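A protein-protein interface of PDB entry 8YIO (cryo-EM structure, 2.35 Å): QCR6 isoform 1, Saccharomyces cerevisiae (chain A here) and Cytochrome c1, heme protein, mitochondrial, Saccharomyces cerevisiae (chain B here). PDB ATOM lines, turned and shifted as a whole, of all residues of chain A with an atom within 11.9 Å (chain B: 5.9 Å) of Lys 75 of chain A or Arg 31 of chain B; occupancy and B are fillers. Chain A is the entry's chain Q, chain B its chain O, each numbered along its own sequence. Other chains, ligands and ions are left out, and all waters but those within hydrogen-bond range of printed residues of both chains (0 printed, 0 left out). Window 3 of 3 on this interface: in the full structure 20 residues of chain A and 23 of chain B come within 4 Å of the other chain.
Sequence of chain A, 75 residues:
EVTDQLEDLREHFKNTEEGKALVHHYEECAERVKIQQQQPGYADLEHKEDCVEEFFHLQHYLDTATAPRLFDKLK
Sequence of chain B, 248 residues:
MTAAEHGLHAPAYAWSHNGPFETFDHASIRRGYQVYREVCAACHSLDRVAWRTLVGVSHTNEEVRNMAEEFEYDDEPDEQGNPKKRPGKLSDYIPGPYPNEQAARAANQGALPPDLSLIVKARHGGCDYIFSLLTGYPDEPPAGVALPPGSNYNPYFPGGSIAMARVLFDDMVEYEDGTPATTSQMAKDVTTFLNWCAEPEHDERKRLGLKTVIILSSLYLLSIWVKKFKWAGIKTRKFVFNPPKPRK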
ATOM      1  N   VAL A   2      -9.123  38.635  -5.454  1.00  0.00           N
ATOM      2  CA  VAL A   2      -9.125  38.656  -6.912  1.00  0.00           C
ATOM      3  C   VAL A   2     -10.494  39.131  -7.376  1.00  0.00           C
ATOM      4  O   VAL A   2     -11.518  38.534  -7.023  1.00  0.00           O
ATOM      5  CB  VAL A   2      -8.796  37.274  -7.501  1.00  0.00           C
ATOM      6  CG1 VAL A   2      -8.877  37.313  -9.021  1.00  0.00           C
ATOM      7  CG2 VAL A   2      -7.422  36.817  -7.048  1.00  0.00           C
ATOM      8  N   THR A   3     -10.511  40.200  -8.163  1.00  0.00           N
ATOM      9  CA  THR A   3     -11.739  40.752  -8.706  1.00  0.00           C
ATOM     10  C   THR A   3     -12.035  40.112 -10.063  1.00  0.00           C
ATOM     11  O   THR A   3     -11.271  39.288 -10.569  1.00  0.00           O
ATOM     12  CB  THR A   3     -11.636  42.276  -8.805  1.00  0.00           C
ATOM     13  OG1 THR A   3     -12.897  42.819  -9.217  1.00  0.00           O
ATOM     14  CG2 THR A   3     -10.558  42.677  -9.795  1.00  0.00           C
ATOM     15  N   ASP A   4     -13.168  40.495 -10.651  1.00  0.00           N
ATOM     16  CA  ASP A   4     -13.639  39.865 -11.878  1.00  0.00           C
ATOM     17  C   ASP A   4     -12.782  40.273 -13.069  1.00  0.00           C
ATOM     18  O   ASP A   4     -12.540  41.462 -13.295  1.00  0.00           O
ATOM     19  CB  ASP A   4     -15.100  40.233 -12.133  1.00  0.00           C
ATOM     20  CG  ASP A   4     -15.752  39.343 -13.175  1.00  0.00           C
ATOM     21  OD1 ASP A   4     -15.173  38.292 -13.511  1.00  0.00           O
ATOM     22  OD2 ASP A   4     -16.847  39.694 -13.657  1.00  0.00           O
ATOM     23  N   GLN A   5     -12.331  39.275 -13.832  1.00  0.00           N
ATOM     24  CA  GLN A   5     -11.476  39.530 -14.988  1.00  0.00           C
ATOM     25  C   GLN A   5     -12.243  40.211 -16.114  1.00  0.00           C
ATOM     26  O   GLN A   5     -11.685  41.054 -16.827  1.00  0.00           O
ATOM     27  CB  GLN A   5     -10.866  38.221 -15.486  1.00  0.00           C
ATOM     28  CG  GLN A   5      -9.595  37.803 -14.782  1.00  0.00           C
ATOM     29  CD  GLN A   5      -9.847  37.251 -13.397  1.00  0.00           C
ATOM     30  OE1 GLN A   5      -9.286  37.734 -12.416  1.00  0.00           O
ATOM     31  NE2 GLN A   5     -10.696  36.237 -13.307  1.00  0.00           N
ATOM     32  N   LEU A   6     -13.515  39.851 -16.301  1.00  0.00           N
ATOM     33  CA  LEU A   6     -14.311  40.457 -17.364  1.00  0.00           C
ATOM     34  C   LEU A   6     -14.664  41.904 -17.046  1.00  0.00           C
ATOM     35  O   LEU A   6     -14.811  42.720 -17.960  1.00  0.00           O
ATOM     36  CB  LEU A   6     -15.581  39.636 -17.599  1.00  0.00           C
ATOM     37  CG  LEU A   6     -16.439  39.935 -18.829  1.00  0.00           C
ATOM     38  CD1 LEU A   6     -15.645  39.758 -20.092  1.00  0.00           C
ATOM     39  CD2 LEU A   6     -17.650  39.035 -18.859  1.00  0.00           C
ATOM     40  N   ARG A  69      -9.072  37.883 -25.745  1.00  0.00           N
ATOM     41  CA  ARG A  69      -8.017  37.981 -24.752  1.00  0.00           C
ATOM     42  C   ARG A  69      -8.458  37.673 -23.327  1.00  0.00           C
ATOM     43  O   ARG A  69      -7.628  37.755 -22.417  1.00  0.00           O
ATOM     44  CB  ARG A  69      -7.386  39.379 -24.786  1.00  0.00           C
ATOM     45  CG  ARG A  69      -8.289  40.476 -24.272  1.00  0.00           C
ATOM     46  CD  ARG A  69      -7.618  41.827 -24.393  1.00  0.00           C
ATOM     47  NE  ARG A  69      -7.389  42.203 -25.783  1.00  0.00           N
ATOM     48  CZ  ARG A  69      -6.694  43.271 -26.160  1.00  0.00           C
ATOM     49  NH1 ARG A  69      -6.534  43.541 -27.448  1.00  0.00           N
ATOM     50  NH2 ARG A  69      -6.159  44.069 -25.248  1.00  0.00           N
ATOM     51  N   LEU A  70      -9.725  37.320 -23.101  1.00  0.00           N
ATOM     52  CA  LEU A  70     -10.186  37.044 -21.745  1.00  0.00           C
ATOM     53  C   LEU A  70      -9.695  35.691 -21.242  1.00  0.00           C
ATOM     54  O   LEU A  70      -9.261  35.575 -20.090  1.00  0.00           O
ATOM     55  CB  LEU A  70     -11.713  37.108 -21.682  1.00  0.00           C
ATOM     56  CG  LEU A  70     -12.365  36.618 -20.384  1.00  0.00           C
ATOM     57  CD1 LEU A  70     -12.042  37.555 -19.234  1.00  0.00           C
ATOM     58  CD2 LEU A  70     -13.867  36.452 -20.537  1.00  0.00           C
ATOM     59  N   PHE A  71      -9.726  34.666 -22.095  1.00  0.00           N
ATOM     60  CA  PHE A  71      -9.449  33.303 -21.654  1.00  0.00           C
ATOM     61  C   PHE A  71      -7.970  33.050 -21.385  1.00  0.00           C
ATOM     62  O   PHE A  71      -7.632  31.996 -20.839  1.00  0.00           O
ATOM     63  CB  PHE A  71      -9.966  32.295 -22.688  1.00  0.00           C
ATOM     64  CG  PHE A  71     -11.422  31.920 -22.519  1.00  0.00           C
ATOM     65  CD1 PHE A  71     -12.342  32.814 -21.986  1.00  0.00           C
ATOM     66  CD2 PHE A  71     -11.870  30.670 -22.912  1.00  0.00           C
ATOM     67  CE1 PHE A  71     -13.668  32.469 -21.843  1.00  0.00           C
ATOM     68  CE2 PHE A  71     -13.196  30.317 -22.774  1.00  0.00           C
ATOM     69  CZ  PHE A  71     -14.097  31.217 -22.237  1.00  0.00           C
ATOM     70  N   ASP A  72      -7.086  33.981 -21.748  1.00  0.00           N
ATOM     71  CA  ASP A  72      -5.687  33.894 -21.351  1.00  0.00           C
ATOM     72  C   ASP A  72      -5.475  34.233 -19.884  1.00  0.00           C
ATOM     73  O   ASP A  72      -4.463  33.824 -19.309  1.00  0.00           O
ATOM     74  CB  ASP A  72      -4.833  34.829 -22.210  1.00  0.00           C
ATOM     75  CG  ASP A  72      -4.447  34.214 -23.532  1.00  0.00           C
ATOM     76  OD1 ASP A  72      -4.125  33.008 -23.557  1.00  0.00           O
ATOM     77  OD2 ASP A  72      -4.465  34.935 -24.549  1.00  0.00           O
ATOM     78  N   LYS A  73      -6.396  34.974 -19.273  1.00  0.00           N
ATOM     79  CA  LYS A  73      -6.287  35.371 -17.877  1.00  0.00           C
ATOM     80  C   LYS A  73      -7.164  34.538 -16.951  1.00  0.00           C
ATOM     81  O   LYS A  73      -7.343  34.910 -15.790  1.00  0.00           O
ATOM     82  CB  LYS A  73      -6.620  36.856 -17.727  1.00  0.00           C
ATOM     83  CG  LYS A  73      -5.595  37.767 -18.377  1.00  0.00           C
ATOM     84  CD  LYS A  73      -5.829  39.225 -18.038  1.00  0.00           C
ATOM     85  CE  LYS A  73      -7.011  39.788 -18.796  1.00  0.00           C
ATOM     86  NZ  LYS A  73      -7.132  41.251 -18.575  1.00  0.00           N
ATOM     87  N   LEU A  74      -7.710  33.426 -17.434  1.00  0.00           N
ATOM     88  CA  LEU A  74      -8.504  32.522 -16.618  1.00  0.00           C
ATOM     89  C   LEU A  74      -7.799  31.178 -16.515  1.00  0.00           C
ATOM     90  O   LEU A  74      -7.117  30.745 -17.448  1.00  0.00           O
ATOM     91  CB  LEU A  74      -9.909  32.325 -17.198  1.00  0.00           C
ATOM     92  CG  LEU A  74     -10.819  33.551 -17.289  1.00  0.00           C
ATOM     93  CD1 LEU A  74     -12.077  33.209 -18.058  1.00  0.00           C
ATOM     94  CD2 LEU A  74     -11.166  34.073 -15.913  1.00  0.00           C
ATOM     95  N   LYS A  75      -7.965  30.520 -15.374  1.00  0.00           N
ATOM     96  CA  LYS A  75      -7.348  29.217 -15.162  1.00  0.00           C
ATOM     97  C   LYS A  75      -8.137  28.134 -15.887  1.00  0.00           C
ATOM     98  O   LYS A  75      -7.576  27.170 -16.402  1.00  0.00           O
ATOM     99  CB  LYS A  75      -7.251  28.899 -13.669  1.00  0.00           C
ATOM    100  CG  LYS A  75      -6.357  27.715 -13.341  1.00  0.00           C
ATOM    101  CD  LYS A  75      -6.411  27.371 -11.861  1.00  0.00           C
ATOM    102  CE  LYS A  75      -5.642  26.100 -11.550  1.00  0.00           C
ATOM    103  NZ  LYS A  75      -6.127  24.948 -12.359  1.00  0.00           N
ATOM    104  OXT LYS A  75      -9.359  28.205 -15.989  1.00  0.00           O
ATOM    105  N   ASP B  25     -10.898  19.934 -21.388  1.00  0.00           N
ATOM    106  CA  ASP B  25     -10.100  20.148 -20.186  1.00  0.00           C
ATOM    107  C   ASP B  25     -10.853  19.510 -19.024  1.00  0.00           C
ATOM    108  O   ASP B  25     -11.891  20.021 -18.593  1.00  0.00           O
ATOM    109  CB  ASP B  25      -9.861  21.638 -19.955  1.00  0.00           C
ATOM    110  CG  ASP B  25      -8.919  21.914 -18.795  1.00  0.00           C
ATOM    111  OD1 ASP B  25      -8.223  20.986 -18.337  1.00  0.00           O
ATOM    112  OD2 ASP B  25      -8.872  23.072 -18.339  1.00  0.00           O
ATOM    113  N   HIS B  26     -10.332  18.394 -18.515  1.00  0.00           N
ATOM    114  CA  HIS B  26     -11.075  17.597 -17.547  1.00  0.00           C
ATOM    115  C   HIS B  26     -11.019  18.159 -16.134  1.00  0.00           C
ATOM    116  O   HIS B  26     -11.854  17.787 -15.305  1.00  0.00           O
ATOM    117  CB  HIS B  26     -10.565  16.157 -17.564  1.00  0.00           C
ATOM    118  CG  HIS B  26     -11.039  15.370 -18.745  1.00  0.00           C
ATOM    119  ND1 HIS B  26     -12.016  14.404 -18.652  1.00  0.00           N
ATOM    120  CD2 HIS B  26     -10.685  15.420 -20.049  1.00  0.00           C
ATOM    121  CE1 HIS B  26     -12.235  13.885 -19.845  1.00  0.00           C
ATOM    122  NE2 HIS B  26     -11.440  14.485 -20.711  1.00  0.00           N
ATOM    123  N   ALA B  27     -10.069  19.046 -15.838  1.00  0.00           N
ATOM    124  CA  ALA B  27     -10.100  19.754 -14.565  1.00  0.00           C
ATOM    125  C   ALA B  27     -11.169  20.838 -14.552  1.00  0.00           C
ATOM    126  O   ALA B  27     -11.743  21.126 -13.497  1.00  0.00           O
ATOM    127  CB  ALA B  27      -8.730  20.361 -14.264  1.00  0.00           C
ATOM    128  N   SER B  28     -11.445  21.441 -15.709  1.00  0.00           N
ATOM    129  CA  SER B  28     -12.541  22.388 -15.846  1.00  0.00           C
ATOM    130  C   SER B  28     -13.904  21.708 -15.831  1.00  0.00           C
ATOM    131  O   SER B  28     -14.891  22.345 -15.454  1.00  0.00           O
ATOM    132  CB  SER B  28     -12.368  23.194 -17.138  1.00  0.00           C
ATOM    133  OG  SER B  28     -13.304  24.250 -17.226  1.00  0.00           O
ATOM    134  N   ILE B  29     -13.979  20.436 -16.229  1.00  0.00           N
ATOM    135  CA  ILE B  29     -15.224  19.682 -16.107  1.00  0.00           C
ATOM    136  C   ILE B  29     -15.519  19.380 -14.642  1.00  0.00           C
ATOM    137  O   ILE B  29     -16.669  19.468 -14.195  1.00  0.00           O
ATOM    138  CB  ILE B  29     -15.151  18.395 -16.954  1.00  0.00           C
ATOM    139  CG1 ILE B  29     -15.031  18.731 -18.439  1.00  0.00           C
ATOM    140  CG2 ILE B  29     -16.371  17.504 -16.739  1.00  0.00           C
ATOM    141  CD1 ILE B  29     -14.867  17.515 -19.320  1.00  0.00           C
ATOM    142  N   ARG B  30     -14.481  19.046 -13.869  1.00  0.00           N
ATOM    143  CA  ARG B  30     -14.658  18.676 -12.467  1.00  0.00           C
ATOM    144  C   ARG B  30     -15.083  19.873 -11.621  1.00  0.00           C
ATOM    145  O   ARG B  30     -15.951  19.744 -10.752  1.00  0.00           O
ATOM    146  CB  ARG B  30     -13.366  18.063 -11.928  1.00  0.00           C
ATOM    147  CG  ARG B  30     -13.416  17.650 -10.471  1.00  0.00           C
ATOM    148  CD  ARG B  30     -12.078  17.110 -10.003  1.00  0.00           C
ATOM    149  NE  ARG B  30     -12.046  16.895  -8.561  1.00  0.00           N
ATOM    150  CZ  ARG B  30     -12.272  15.727  -7.970  1.00  0.00           C
ATOM    151  NH1 ARG B  30     -12.221  15.631  -6.653  1.00  0.00           N
ATOM    152  NH2 ARG B  30     -12.552  14.656  -8.694  1.00  0.00           N
ATOM    153  N   ARG B  31     -14.496  21.044 -11.873  1.00  0.00           N
ATOM    154  CA  ARG B  31     -14.939  22.258 -11.195  1.00  0.00           C
ATOM    155  C   ARG B  31     -16.325  22.685 -11.657  1.00  0.00           C
ATOM    156  O   ARG B  31     -17.064  23.307 -10.890  1.00  0.00           O
ATOM    157  CB  ARG B  31     -13.941  23.391 -11.428  1.00  0.00           C
ATOM    158  CG  ARG B  31     -12.652  23.274 -10.640  1.00  0.00           C
ATOM    159  CD  ARG B  31     -11.837  24.550 -10.731  1.00  0.00           C
ATOM    160  NE  ARG B  31     -11.651  24.983 -12.112  1.00  0.00           N
ATOM    161  CZ  ARG B  31     -10.588  24.697 -12.853  1.00  0.00           C
ATOM    162  NH1 ARG B  31     -10.512  25.135 -14.099  1.00  0.00           N
ATOM    163  NH2 ARG B  31      -9.600  23.975 -12.350  1.00  0.00           N
ATOM    164  N   GLY B  32     -16.690  22.357 -12.898  1.00  0.00           N
ATOM    165  CA  GLY B  32     -17.993  22.736 -13.411  1.00  0.00           C
ATOM    166  C   GLY B  32     -19.140  21.971 -12.787  1.00  0.00           C
ATOM    167  O   GLY B  32     -20.249  22.498 -12.681  1.00  0.00           O
ATOM    168  N   TYR B  33     -18.900  20.721 -12.376  1.00  0.00           N
ATOM    169  CA  TYR B  33     -19.927  19.960 -11.671  1.00  0.00           C
ATOM    170  C   TYR B  33     -20.214  20.549 -10.294  1.00  0.00           C
ATOM    171  O   TYR B  33     -21.351  20.472  -9.818  1.00  0.00           O
ATOM    172  CB  TYR B  33     -19.518  18.485 -11.544  1.00  0.00           C
ATOM    173  CG  TYR B  33     -20.515  17.653 -10.758  1.00  0.00           C
ATOM    174  CD1 TYR B  33     -21.702  17.235 -11.340  1.00  0.00           C
ATOM    175  CD2 TYR B  33     -20.281  17.316  -9.427  1.00  0.00           C
ATOM    176  CE1 TYR B  33     -22.622  16.502 -10.629  1.00  0.00           C
ATOM    177  CE2 TYR B  33     -21.199  16.588  -8.708  1.00  0.00           C
ATOM    178  CZ  TYR B  33     -22.367  16.181  -9.316  1.00  0.00           C
ATOM    179  OH  TYR B  33     -23.282  15.446  -8.609  1.00  0.00           O
ATOM    180  N   GLN B  34     -19.203  21.126  -9.640  1.00  0.00           N
ATOM    181  CA  GLN B  34     -19.412  21.727  -8.328  1.00  0.00           C
ATOM    182  C   GLN B  34     -20.275  22.980  -8.411  1.00  0.00           C
ATOM    183  O   GLN B  34     -21.049  23.258  -7.491  1.00  0.00           O
ATOM    184  CB  GLN B  34     -18.066  22.045  -7.676  1.00  0.00           C
ATOM    185  CG  GLN B  34     -18.148  22.327  -6.190  1.00  0.00           C
ATOM    186  CD  GLN B  34     -16.815  22.727  -5.594  1.00  0.00           C
ATOM    187  OE1 GLN B  34     -15.772  22.576  -6.222  1.00  0.00           O
ATOM    188  NE2 GLN B  34     -16.846  23.243  -4.377  1.00  0.00           N
ATOM    189  N   VAL B  35     -20.170  23.734  -9.508  1.00  0.00           N
ATOM    190  CA  VAL B  35     -21.059  24.870  -9.723  1.00  0.00           C
ATOM    191  C   VAL B  35     -22.479  24.392 -10.013  1.00  0.00           C
ATOM    192  O   VAL B  35     -23.452  25.083  -9.685  1.00  0.00           O
ATOM    193  CB  VAL B  35     -20.505  25.769 -10.848  1.00  0.00           C
ATOM    194  CG1 VAL B  35     -21.239  27.100 -10.909  1.00  0.00           C
ATOM    195  CG2 VAL B  35     -19.023  26.016 -10.645  1.00  0.00           C
ATOM    196  N   TYR B  36     -22.632  23.201 -10.600  1.00  0.00           N
ATOM    197  CA  TYR B  36     -23.973  22.682 -10.847  1.00  0.00           C
ATOM    198  C   TYR B  36     -24.667  22.279  -9.552  1.00  0.00           C
ATOM    199  O   TYR B  36     -25.850  22.574  -9.365  1.00  0.00           O
ATOM    200  CB  TYR B  36     -23.938  21.500 -11.819  1.00  0.00           C
ATOM    201  CG  TYR B  36     -25.283  20.813 -11.938  1.00  0.00           C
ATOM    202  CD1 TYR B  36     -26.327  21.417 -12.623  1.00  0.00           C
ATOM    203  CD2 TYR B  36     -25.516  19.574 -11.346  1.00  0.00           C
ATOM    204  CE1 TYR B  36     -27.562  20.813 -12.719  1.00  0.00           C
ATOM    205  CE2 TYR B  36     -26.747  18.965 -11.433  1.00  0.00           C
ATOM    206  CZ  TYR B  36     -27.764  19.587 -12.124  1.00  0.00           C
ATOM    207  OH  TYR B  36     -28.991  18.982 -12.223  1.00  0.00           O
ATOM    208  N   TYR B 175     -13.562  26.318  -4.071  1.00  0.00           N
ATOM    209  CA  TYR B 175     -13.046  25.266  -4.937  1.00  0.00           C
ATOM    210  C   TYR B 175     -12.084  24.355  -4.183  1.00  0.00           C
ATOM    211  O   TYR B 175     -11.459  24.752  -3.198  1.00  0.00           O
ATOM    212  CB  TYR B 175     -12.335  25.865  -6.149  1.00  0.00           C
ATOM    213  CG  TYR B 175     -13.249  26.212  -7.302  1.00  0.00           C
ATOM    214  CD1 TYR B 175     -14.279  25.360  -7.681  1.00  0.00           C
ATOM    215  CD2 TYR B 175     -13.076  27.389  -8.015  1.00  0.00           C
ATOM    216  CE1 TYR B 175     -15.114  25.676  -8.736  1.00  0.00           C
ATOM    217  CE2 TYR B 175     -13.900  27.713  -9.068  1.00  0.00           C
ATOM    218  CZ  TYR B 175     -14.917  26.854  -9.425  1.00  0.00           C
ATOM    219  OH  TYR B 175     -15.736  27.181 -10.475  1.00  0.00           O
ATOM    220  N   ASP B 177      -9.342  22.658  -5.617  1.00  0.00           N
ATOM    221  CA  ASP B 177      -7.959  22.822  -6.048  1.00  0.00           C
ATOM    222  C   ASP B 177      -7.399  24.212  -5.770  1.00  0.00           C
ATOM    223  O   ASP B 177      -6.209  24.437  -6.011  1.00  0.00           O
ATOM    224  CB  ASP B 177      -7.833  22.500  -7.541  1.00  0.00           C
ATOM    225  CG  ASP B 177      -7.989  21.021  -7.839  1.00  0.00           C
ATOM    226  OD1 ASP B 177      -7.912  20.209  -6.897  1.00  0.00           O
ATOM    227  OD2 ASP B 177      -8.198  20.670  -9.017  1.00  0.00           O
ATOM    228  N   THR B 179      -8.693  27.362  -6.944  1.00  0.00           N
ATOM    229  CA  THR B 179      -8.874  28.386  -7.962  1.00  0.00           C
ATOM    230  C   THR B 179      -9.709  29.536  -7.399  1.00  0.00           C
ATOM    231  O   THR B 179     -10.679  29.295  -6.670  1.00  0.00           O
ATOM    232  CB  THR B 179      -9.561  27.778  -9.188  1.00  0.00           C
ATOM    233  OG1 THR B 179      -8.898  26.562  -9.551  1.00  0.00           O
ATOM    234  CG2 THR B 179      -9.542  28.728 -10.376  1.00  0.00           C
ATOM    235  N   PRO B 180      -9.346  30.792  -7.684  1.00  0.00           N
ATOM    236  CA  PRO B 180     -10.217  31.916  -7.307  1.00  0.00           C
ATOM    237  C   PRO B 180     -11.532  31.875  -8.073  1.00  0.00           C
ATOM    238  O   PRO B 180     -11.549  31.788  -9.301  1.00  0.00           O
ATOM    239  CB  PRO B 180      -9.389  33.151  -7.681  1.00  0.00           C
ATOM    240  CG  PRO B 180      -7.989  32.675  -7.730  1.00  0.00           C
ATOM    241  CD  PRO B 180      -8.041  31.254  -8.183  1.00  0.00           C
ATOM    242  N   GLN B 185     -14.808  32.982 -13.987  1.00  0.00           N
ATOM    243  CA  GLN B 185     -14.243  31.644 -13.862  1.00  0.00           C
ATOM    244  C   GLN B 185     -15.335  30.595 -13.685  1.00  0.00           C
ATOM    245  O   GLN B 185     -15.257  29.507 -14.266  1.00  0.00           O
ATOM    246  CB  GLN B 185     -13.257  31.604 -12.694  1.00  0.00           C
ATOM    247  CG  GLN B 185     -12.596  30.259 -12.474  1.00  0.00           C
ATOM    248  CD  GLN B 185     -11.533  29.955 -13.503  1.00  0.00           C
ATOM    249  OE1 GLN B 185     -10.527  30.653 -13.594  1.00  0.00           O
ATOM    250  NE2 GLN B 185     -11.748  28.907 -14.283  1.00  0.00           N
ATOM    251  N   LYS B 188     -17.228  29.954 -16.979  1.00  0.00           N
ATOM    252  CA  LYS B 188     -16.445  29.190 -17.943  1.00  0.00           C
ATOM    253  C   LYS B 188     -16.446  27.705 -17.603  1.00  0.00           C
ATOM    254  O   LYS B 188     -16.502  26.858 -18.502  1.00  0.00           O
ATOM    255  CB  LYS B 188     -15.018  29.738 -17.990  1.00  0.00           C
ATOM    256  CG  LYS B 188     -14.062  28.970 -18.880  1.00  0.00           C
ATOM    257  CD  LYS B 188     -12.661  29.533 -18.793  1.00  0.00           C
ATOM    258  CE  LYS B 188     -11.637  28.532 -19.280  1.00  0.00           C
ATOM    259  NZ  LYS B 188     -11.541  27.363 -18.370  1.00  0.00           N
ATOM    260  N   ASP B 189     -16.411  27.372 -16.310  1.00  0.00           N
ATOM    261  CA  ASP B 189     -16.324  25.975 -15.899  1.00  0.00           C
ATOM    262  C   ASP B 189     -17.642  25.242 -16.106  1.00  0.00           C
ATOM    263  O   ASP B 189     -17.648  24.089 -16.550  1.00  0.00           O
ATOM    264  CB  ASP B 189     -15.888  25.885 -14.435  1.00  0.00           C
ATOM    265  CG  ASP B 189     -14.434  26.251 -14.236  1.00  0.00           C
ATOM    266  OD1 ASP B 189     -13.630  26.027 -15.160  1.00  0.00           O
ATOM    267  OD2 ASP B 189     -14.091  26.764 -13.154  1.00  0.00           O
ATOM    268  N   VAL B 190     -18.767  25.886 -15.792  1.00  0.00           N
ATOM    269  CA  VAL B 190     -20.054  25.211 -15.913  1.00  0.00           C
ATOM    270  C   VAL B 190     -20.490  25.089 -17.373  1.00  0.00           C
ATOM    271  O   VAL B 190     -21.248  24.173 -17.709  1.00  0.00           O
ATOM    272  CB  VAL B 190     -21.105  25.922 -15.032  1.00  0.00           C
ATOM    273  CG1 VAL B 190     -21.522  27.271 -15.606  1.00  0.00           C
ATOM    274  CG2 VAL B 190     -22.308  25.026 -14.748  1.00  0.00           C
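OXT of Lys 75 of chain A lies within salt-bridge range of NH1 of Arg 31 of chain B, 3.8 Å away.
NE2 of Gln 185 of chain B lies within hydrogen-bond range of OXT of Lys 75 of chain A (3.0 Å).
The chain-end carboxylate (OXT) of Lys 75 of chain A lies within salt-bridge range of the side-chain amino group (NZ) of Lys 188 of chain B (3.3 Å).
NE of Arg 31 of chain B is in salt-bridge range of OD2 of Asp 189 of chain B (3.2 Å).
NE2 of Gln 185 of chain B is in hydrogen-bond range of OD2 of Asp 189 of chain B (3.4 Å).
Among the printed residues, pairs that only touch across the chains: Leu 74 of chain A with Lys 188 of chain B and Lys 75 of chain A with Thr 179 of chain B.
Printed residues of chain A that touch a printed residue of chain B: Leu 74 and Lys 75.
Hydrophobic or aromatic side chains of chain A within 4 Å of the printed part of chain B: Leu 74.
Printed residues of chain B that touch a printed residue of chain A: Arg 31, Thr 179, Gln 185 and Lys 188.
Among the printed residues, 5 pairs touch across the chains.
Among the printed residues, no Asp or Glu carboxylate lies within 4 Å of a Lys or Arg side-chain nitrogen of the other chain.
Printed residues of chain B within 4 Å of Leu 74 of chain A: Lys 188.
Of the printed residues of chain B, Lys 75 of chain A touches Arg 31, Thr 179, Gln 185 and Lys 188.
No residue of chain A comes within 4 Å of Ala 27 of chain B.
Ile 29 of chain B touches none of the printed residues of chain A.
Arg 31 of chain B touches one residue of chain A.
No residue of chain A comes within 4 Å of Gly 32 of chain B.
No residue of chain A comes within 4 Å of Gln 34 of chain B.
No residue of chain A comes within 4 Å of Tyr 175 of chain B.
No residue of chain A comes within 4 Å of Asp 177 of chain B.
Of chain A, only Lys 75 comes within 4 Å of Thr 179 of chain B.
No residue of chain A comes within 4 Å of Pro 180 of chain B.
Gln 185 of chain B touches one residue of chain A.
Printed residues of chain A within 4 Å of Lys 188 of chain B: Leu 74 and Lys 75.
No residue of chain A comes within 4 Å of Asp 189 of chain B.
Val 190 of chain B touches none of the printed residues of chain A.
The nearest residue of chain B that does not touch Lys 75 of chain A is Asp 25 of chain B (4.7 Å).
The nearest printed residue of chain B that does not touch Leu 74 of chain A is Gln 185 of chain B (4.02 Å).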
